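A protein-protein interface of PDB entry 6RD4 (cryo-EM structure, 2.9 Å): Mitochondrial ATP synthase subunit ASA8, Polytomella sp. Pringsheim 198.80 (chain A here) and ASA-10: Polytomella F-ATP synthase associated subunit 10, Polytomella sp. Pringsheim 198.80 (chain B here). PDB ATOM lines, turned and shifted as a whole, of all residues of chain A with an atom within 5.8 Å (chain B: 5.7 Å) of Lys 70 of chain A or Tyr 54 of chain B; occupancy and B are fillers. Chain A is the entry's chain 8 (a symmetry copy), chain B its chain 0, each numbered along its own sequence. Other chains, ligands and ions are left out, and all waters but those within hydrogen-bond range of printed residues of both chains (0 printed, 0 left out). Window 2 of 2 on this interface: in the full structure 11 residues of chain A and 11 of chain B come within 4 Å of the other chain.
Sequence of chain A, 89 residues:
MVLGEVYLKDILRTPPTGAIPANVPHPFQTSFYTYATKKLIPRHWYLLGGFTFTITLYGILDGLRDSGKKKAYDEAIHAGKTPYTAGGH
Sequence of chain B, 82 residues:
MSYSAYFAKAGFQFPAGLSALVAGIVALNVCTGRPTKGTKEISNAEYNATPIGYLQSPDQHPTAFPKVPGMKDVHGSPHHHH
OH of Tyr 54 of chain B lies close to NZ of Lys 70 of chain A.
N of Ile 52 of chain B lies close to OD2 of Asp 66 of chain A (2.8 Å).
The side-chain hydroxyl (OH) of Tyr 54 of chain B sits at hydrogen-bond distance from the side-chain carboxylate (OD1) of Asp 74 of chain A (3.3 Å).
The side-chain amino group of Lys 70 of chain A lies within salt-bridge range of the side-chain carboxylate of Asp 74 of chain A, 3.3 Å away.
The backbone NH (N) of His 79 of chain B sits close to the side-chain hydroxyl (OG) of Ser 77 of chain B, at 3.3 Å.
Among the printed residues, merely in contact across the chains: Asp 74 of chain A with His 79 of chain B (3.1 Å), Lys 70 of chain A with Pro 51 of chain B (3.4 Å), Tyr 73 of chain A with Tyr 54 of chain B (3.6 Å), Lys 69 of chain A with Thr 50 of chain B (3.8 Å), Asp 66 of chain A with Pro 51 of chain B (3.8 Å) and Lys 69 of chain A with Pro 51 of chain B (3.9 Å).
Lys 70 of chain A touches just these residues of chain B: Pro 51 and Tyr 54.
Of the printed residues of chain B, Lys 69 of chain A touches Thr 50 and Pro 51.
Of the printed residues of chain B, Asp 66 of chain A touches Pro 51 and Ile 52.
Of the printed residues of chain B, Asp 74 of chain A touches Tyr 54 and His 79.
Of the printed residues of chain A, Ile 52 of chain B touches Asp 66.
Ala 72 of chain A touches none of the printed residues of chain B.
Lys 71 of chain A touches none of the printed residues of chain B.
The nearest printed residue of chain B that does not touch Lys 70 of chain A is Thr 50 of chain B (6.1 Å).
The nearest printed residue of chain A that does not touch Tyr 54 of chain B is Lys 69 of chain A (6.5 Å).
Of the 12 printed residues of chain B, 5 touch a printed residue of chain A.
Hydrophobic or aromatic side chains of chain B that line the printed part of chain A: Pro 51, Ile 52, Tyr 54 and His 79.
Along chain B the printed residues that touch a printed residue of chain A span positions 50 to 79.
Of the 11 printed residues of chain A, 5 touch a printed residue of chain B.
Printed residues of chain A that touch a printed residue of chain B: Asp 66, Lys 69, Lys 70, Tyr 73 and Asp 74.
Hydrophobic or aromatic side chains of chain A that line the printed part of chain B: Tyr 73.
Among the printed residues, no Asp or Glu carboxylate lies within 4 Å of a Lys or Arg side-chain nitrogen of the other chain.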
ATOM      1  N   ARG A  65      18.425  -2.435 -27.808  1.00  0.00           N
ATOM      2  CA  ARG A  65      19.287  -2.100 -26.690  1.00  0.00           C
ATOM      3  C   ARG A  65      18.543  -1.322 -25.619  1.00  0.00           C
ATOM      4  O   ARG A  65      18.841  -1.467 -24.435  1.00  0.00           O
ATOM      5  CB  ARG A  65      20.488  -1.313 -27.187  1.00  0.00           C
ATOM      6  CG  ARG A  65      21.564  -1.140 -26.173  1.00  0.00           C
ATOM      7  CD  ARG A  65      22.898  -1.143 -26.823  1.00  0.00           C
ATOM      8  NE  ARG A  65      23.041  -0.022 -27.732  1.00  0.00           N
ATOM      9  CZ  ARG A  65      23.722   1.077 -27.443  1.00  0.00           C
ATOM     10  NH1 ARG A  65      23.807   2.054 -28.332  1.00  0.00           N
ATOM     11  NH2 ARG A  65      24.322   1.196 -26.270  1.00  0.00           N
ATOM     12  N   ASP A  66      17.579  -0.489 -25.998  1.00  0.00           N
ATOM     13  CA  ASP A  66      16.768   0.195 -25.000  1.00  0.00           C
ATOM     14  C   ASP A  66      15.607  -0.629 -24.489  1.00  0.00           C
ATOM     15  O   ASP A  66      15.156  -0.390 -23.371  1.00  0.00           O
ATOM     16  CB  ASP A  66      16.216   1.516 -25.525  1.00  0.00           C
ATOM     17  CG  ASP A  66      17.074   2.697 -25.139  1.00  0.00           C
ATOM     18  OD1 ASP A  66      18.299   2.542 -24.954  1.00  0.00           O
ATOM     19  OD2 ASP A  66      16.510   3.796 -24.998  1.00  0.00           O
ATOM     20  N   SER A  67      15.105  -1.586 -25.253  1.00  0.00           N
ATOM     21  CA  SER A  67      14.137  -2.495 -24.671  1.00  0.00           C
ATOM     22  C   SER A  67      14.801  -3.520 -23.771  1.00  0.00           C
ATOM     23  O   SER A  67      14.113  -4.174 -22.991  1.00  0.00           O
ATOM     24  CB  SER A  67      13.331  -3.197 -25.754  1.00  0.00           C
ATOM     25  OG  SER A  67      14.137  -4.097 -26.474  1.00  0.00           O
ATOM     26  N   GLY A  68      16.115  -3.689 -23.876  1.00  0.00           N
ATOM     27  CA  GLY A  68      16.846  -4.470 -22.904  1.00  0.00           C
ATOM     28  C   GLY A  68      17.322  -3.676 -21.714  1.00  0.00           C
ATOM     29  O   GLY A  68      17.636  -4.265 -20.682  1.00  0.00           O
ATOM     30  N   LYS A  69      17.430  -2.362 -21.850  1.00  0.00           N
ATOM     31  CA  LYS A  69      17.692  -1.506 -20.703  1.00  0.00           C
ATOM     32  C   LYS A  69      16.442  -1.326 -19.872  1.00  0.00           C
ATOM     33  O   LYS A  69      16.515  -1.234 -18.649  1.00  0.00           O
ATOM     34  CB  LYS A  69      18.183  -0.141 -21.162  1.00  0.00           C
ATOM     35  CG  LYS A  69      19.659   0.029 -21.278  1.00  0.00           C
ATOM     36  CD  LYS A  69      19.920   1.417 -21.767  1.00  0.00           C
ATOM     37  CE  LYS A  69      21.371   1.756 -21.754  1.00  0.00           C
ATOM     38  NZ  LYS A  69      21.538   3.157 -22.184  1.00  0.00           N
ATOM     39  N   LYS A  70      15.295  -1.229 -20.532  1.00  0.00           N
ATOM     40  CA  LYS A  70      14.028  -1.085 -19.837  1.00  0.00           C
ATOM     41  C   LYS A  70      13.650  -2.362 -19.123  1.00  0.00           C
ATOM     42  O   LYS A  70      13.030  -2.313 -18.060  1.00  0.00           O
ATOM     43  CB  LYS A  70      12.952  -0.700 -20.841  1.00  0.00           C
ATOM     44  CG  LYS A  70      11.627  -0.336 -20.271  1.00  0.00           C
ATOM     45  CD  LYS A  70      10.668  -0.017 -21.390  1.00  0.00           C
ATOM     46  CE  LYS A  70       9.283   0.281 -20.863  1.00  0.00           C
ATOM     47  NZ  LYS A  70       8.739  -0.860 -20.091  1.00  0.00           N
ATOM     48  N   LYS A  71      14.019  -3.509 -19.682  1.00  0.00           N
ATOM     49  CA  LYS A  71      13.745  -4.778 -19.024  1.00  0.00           C
ATOM     50  C   LYS A  71      14.587  -4.941 -17.770  1.00  0.00           C
ATOM     51  O   LYS A  71      14.083  -5.383 -16.738  1.00  0.00           O
ATOM     52  CB  LYS A  71      13.973  -5.919 -20.010  1.00  0.00           C
ATOM     53  CG  LYS A  71      14.420  -7.226 -19.412  1.00  0.00           C
ATOM     54  CD  LYS A  71      14.381  -8.324 -20.450  1.00  0.00           C
ATOM     55  CE  LYS A  71      15.184  -9.527 -20.018  1.00  0.00           C
ATOM     56  NZ  LYS A  71      14.739 -10.060 -18.714  1.00  0.00           N
ATOM     57  N   ALA A  72      15.848  -4.549 -17.812  1.00  0.00           N
ATOM     58  CA  ALA A  72      16.675  -4.637 -16.621  1.00  0.00           C
ATOM     59  C   ALA A  72      16.422  -3.513 -15.635  1.00  0.00           C
ATOM     60  O   ALA A  72      16.846  -3.617 -14.485  1.00  0.00           O
ATOM     61  CB  ALA A  72      18.151  -4.651 -17.002  1.00  0.00           C
ATOM     62  N   TYR A  73      15.778  -2.430 -16.057  1.00  0.00           N
ATOM     63  CA  TYR A  73      15.471  -1.339 -15.140  1.00  0.00           C
ATOM     64  C   TYR A  73      14.234  -1.646 -14.325  1.00  0.00           C
ATOM     65  O   TYR A  73      14.214  -1.419 -13.114  1.00  0.00           O
ATOM     66  CB  TYR A  73      15.265  -0.046 -15.911  1.00  0.00           C
ATOM     67  CG  TYR A  73      15.365   1.216 -15.108  1.00  0.00           C
ATOM     68  CD1 TYR A  73      16.584   1.808 -14.876  1.00  0.00           C
ATOM     69  CD2 TYR A  73      14.238   1.840 -14.627  1.00  0.00           C
ATOM     70  CE1 TYR A  73      16.682   2.970 -14.168  1.00  0.00           C
ATOM     71  CE2 TYR A  73      14.329   3.000 -13.913  1.00  0.00           C
ATOM     72  CZ  TYR A  73      15.557   3.559 -13.687  1.00  0.00           C
ATOM     73  OH  TYR A  73      15.660   4.721 -12.975  1.00  0.00           O
ATOM     74  N   ASP A  74      13.196  -2.163 -14.977  1.00  0.00           N
ATOM     75  CA  ASP A  74      11.982  -2.540 -14.274  1.00  0.00           C
ATOM     76  C   ASP A  74      12.223  -3.702 -13.330  1.00  0.00           C
ATOM     77  O   ASP A  74      11.604  -3.771 -12.269  1.00  0.00           O
ATOM     78  CB  ASP A  74      10.902  -2.904 -15.279  1.00  0.00           C
ATOM     79  CG  ASP A  74      10.582  -1.776 -16.200  1.00  0.00           C
ATOM     80  OD1 ASP A  74      11.137  -0.684 -15.998  1.00  0.00           O
ATOM     81  OD2 ASP A  74       9.781  -1.979 -17.129  1.00  0.00           O
ATOM     82  N   GLU A  75      13.150  -4.587 -13.663  1.00  0.00           N
ATOM     83  CA  GLU A  75      13.474  -5.720 -12.816  1.00  0.00           C
ATOM     84  C   GLU A  75      14.392  -5.360 -11.665  1.00  0.00           C
ATOM     85  O   GLU A  75      14.926  -6.262 -11.021  1.00  0.00           O
ATOM     86  CB  GLU A  75      14.114  -6.822 -13.648  1.00  0.00           C
ATOM     87  CG  GLU A  75      13.140  -7.572 -14.508  1.00  0.00           C
ATOM     88  CD  GLU A  75      13.837  -8.411 -15.547  1.00  0.00           C
ATOM     89  OE1 GLU A  75      13.227  -8.680 -16.602  1.00  0.00           O
ATOM     90  OE2 GLU A  75      15.000  -8.794 -15.312  1.00  0.00           O
ATOM     91  N   THR B  50      19.511   3.860 -17.850  1.00  0.00           N
ATOM     92  CA  THR B  50      18.132   4.280 -18.013  1.00  0.00           C
ATOM     93  C   THR B  50      17.735   4.223 -19.478  1.00  0.00           C
ATOM     94  O   THR B  50      18.522   4.616 -20.340  1.00  0.00           O
ATOM     95  CB  THR B  50      17.961   5.706 -17.497  1.00  0.00           C
ATOM     96  OG1 THR B  50      18.631   5.839 -16.241  1.00  0.00           O
ATOM     97  CG2 THR B  50      16.527   6.029 -17.268  1.00  0.00           C
ATOM     98  N   PRO B  51      16.548   3.722 -19.806  1.00  0.00           N
ATOM     99  CA  PRO B  51      16.052   3.835 -21.179  1.00  0.00           C
ATOM    100  C   PRO B  51      15.815   5.286 -21.561  1.00  0.00           C
ATOM    101  O   PRO B  51      15.615   6.153 -20.713  1.00  0.00           O
ATOM    102  CB  PRO B  51      14.727   3.075 -21.141  1.00  0.00           C
ATOM    103  CG  PRO B  51      14.786   2.253 -19.961  1.00  0.00           C
ATOM    104  CD  PRO B  51      15.663   2.902 -18.974  1.00  0.00           C
ATOM    105  N   ILE B  52      15.809   5.544 -22.870  1.00  0.00           N
ATOM    106  CA  ILE B  52      15.553   6.905 -23.328  1.00  0.00           C
ATOM    107  C   ILE B  52      14.093   7.277 -23.197  1.00  0.00           C
ATOM    108  O   ILE B  52      13.757   8.452 -23.308  1.00  0.00           O
ATOM    109  CB  ILE B  52      15.999   7.137 -24.778  1.00  0.00           C
ATOM    110  CG1 ILE B  52      15.269   6.190 -25.723  1.00  0.00           C
ATOM    111  CG2 ILE B  52      17.500   6.993 -24.905  1.00  0.00           C
ATOM    112  CD1 ILE B  52      15.607   6.417 -27.172  1.00  0.00           C
ATOM    113  N   GLY B  53      13.203   6.310 -22.998  1.00  0.00           N
ATOM    114  CA  GLY B  53      11.838   6.650 -22.655  1.00  0.00           C
ATOM    115  C   GLY B  53      11.641   7.016 -21.208  1.00  0.00           C
ATOM    116  O   GLY B  53      10.619   7.610 -20.868  1.00  0.00           O
ATOM    117  N   TYR B  54      12.590   6.665 -20.346  1.00  0.00           N
ATOM    118  CA  TYR B  54      12.496   6.981 -18.931  1.00  0.00           C
ATOM    119  C   TYR B  54      13.338   8.176 -18.549  1.00  0.00           C
ATOM    120  O   TYR B  54      13.145   8.727 -17.464  1.00  0.00           O
ATOM    121  CB  TYR B  54      12.935   5.798 -18.060  1.00  0.00           C
ATOM    122  CG  TYR B  54      11.975   4.631 -17.979  1.00  0.00           C
ATOM    123  CD1 TYR B  54      10.791   4.618 -18.696  1.00  0.00           C
ATOM    124  CD2 TYR B  54      12.257   3.542 -17.168  1.00  0.00           C
ATOM    125  CE1 TYR B  54       9.936   3.560 -18.626  1.00  0.00           C
ATOM    126  CE2 TYR B  54      11.396   2.482 -17.086  1.00  0.00           C
ATOM    127  CZ  TYR B  54      10.238   2.502 -17.818  1.00  0.00           C
ATOM    128  OH  TYR B  54       9.363   1.454 -17.760  1.00  0.00           O
ATOM    129  N   LEU B  55      14.283   8.569 -19.395  1.00  0.00           N
ATOM    130  CA  LEU B  55      14.969   9.834 -19.188  1.00  0.00           C
ATOM    131  C   LEU B  55      14.063  11.005 -19.511  1.00  0.00           C
ATOM    132  O   LEU B  55      14.231  12.088 -18.951  1.00  0.00           O
ATOM    133  CB  LEU B  55      16.215   9.902 -20.049  1.00  0.00           C
ATOM    134  CG  LEU B  55      17.316   8.911 -19.747  1.00  0.00           C
ATOM    135  CD1 LEU B  55      18.183   8.802 -20.951  1.00  0.00           C
ATOM    136  CD2 LEU B  55      18.118   9.334 -18.562  1.00  0.00           C
ATOM    137  N   GLN B  56      13.108  10.809 -20.407  1.00  0.00           N
ATOM    138  CA  GLN B  56      12.195  11.870 -20.789  1.00  0.00           C
ATOM    139  C   GLN B  56      11.162  12.134 -19.709  1.00  0.00           C
ATOM    140  O   GLN B  56      10.627  11.212 -19.101  1.00  0.00           O
ATOM    141  CB  GLN B  56      11.488  11.504 -22.077  1.00  0.00           C
ATOM    142  CG  GLN B  56      12.398  11.460 -23.251  1.00  0.00           C
ATOM    143  CD  GLN B  56      11.723  10.896 -24.454  1.00  0.00           C
ATOM    144  OE1 GLN B  56      10.619  10.378 -24.365  1.00  0.00           O
ATOM    145  NE2 GLN B  56      12.376  10.994 -25.594  1.00  0.00           N
ATOM    146  N   SER B  57      10.888  13.339 -19.497  1.00  0.00           N
ATOM    147  CA  SER B  57       9.832  13.762 -18.607  1.00  0.00           C
ATOM    148  C   SER B  57       8.578  14.056 -19.409  1.00  0.00           C
ATOM    149  O   SER B  57       8.662  14.371 -20.593  1.00  0.00           O
ATOM    150  CB  SER B  57      10.239  15.015 -17.841  1.00  0.00           C
ATOM    151  OG  SER B  57      11.408  14.796 -17.077  1.00  0.00           O
ATOM    152  N   GLY B  76       7.192   8.876 -19.757  1.00  0.00           N
ATOM    153  CA  GLY B  76       8.306   8.835 -18.847  1.00  0.00           C
ATOM    154  C   GLY B  76       8.304   7.613 -17.951  1.00  0.00           C
ATOM    155  O   GLY B  76       7.683   6.585 -18.225  1.00  0.00           O
ATOM    156  N   SER B  77       9.017   7.753 -16.847  1.00  0.00           N
ATOM    157  CA  SER B  77       9.205   6.657 -15.922  1.00  0.00           C
ATOM    158  C   SER B  77       7.940   6.463 -15.101  1.00  0.00           C
ATOM    159  O   SER B  77       7.481   7.414 -14.461  1.00  0.00           O
ATOM    160  CB  SER B  77      10.387   6.943 -15.011  1.00  0.00           C
ATOM    161  OG  SER B  77      10.631   5.873 -14.124  1.00  0.00           O
ATOM    162  N   PRO B  78       7.341   5.269 -15.093  1.00  0.00           N
ATOM    163  CA  PRO B  78       6.233   5.007 -14.172  1.00  0.00           C
ATOM    164  C   PRO B  78       6.698   4.708 -12.765  1.00  0.00           C
ATOM    165  O   PRO B  78       5.857   4.565 -11.868  1.00  0.00           O
ATOM    166  CB  PRO B  78       5.551   3.793 -14.794  1.00  0.00           C
ATOM    167  CG  PRO B  78       6.664   3.063 -15.420  1.00  0.00           C
ATOM    168  CD  PRO B  78       7.635   4.095 -15.924  1.00  0.00           C
ATOM    169  N   HIS B  79       8.007   4.612 -12.551  1.00  0.00           N
ATOM    170  CA  HIS B  79       8.582   4.384 -11.231  1.00  0.00           C
ATOM    171  C   HIS B  79       8.710   5.714 -10.496  1.00  0.00           C
ATOM    172  O   HIS B  79       9.793   6.267 -10.299  1.00  0.00           O
ATOM    173  CB  HIS B  79       9.920   3.679 -11.360  1.00  0.00           C
ATOM    174  CG  HIS B  79       9.833   2.381 -12.086  1.00  0.00           C
ATOM    175  ND1 HIS B  79       9.877   2.295 -13.460  1.00  0.00           N
ATOM    176  CD2 HIS B  79       9.668   1.117 -11.634  1.00  0.00           C
ATOM    177  CE1 HIS B  79       9.759   1.032 -13.822  1.00  0.00           C
ATOM    178  NE2 HIS B  79       9.629   0.296 -12.733  1.00  0.00           N
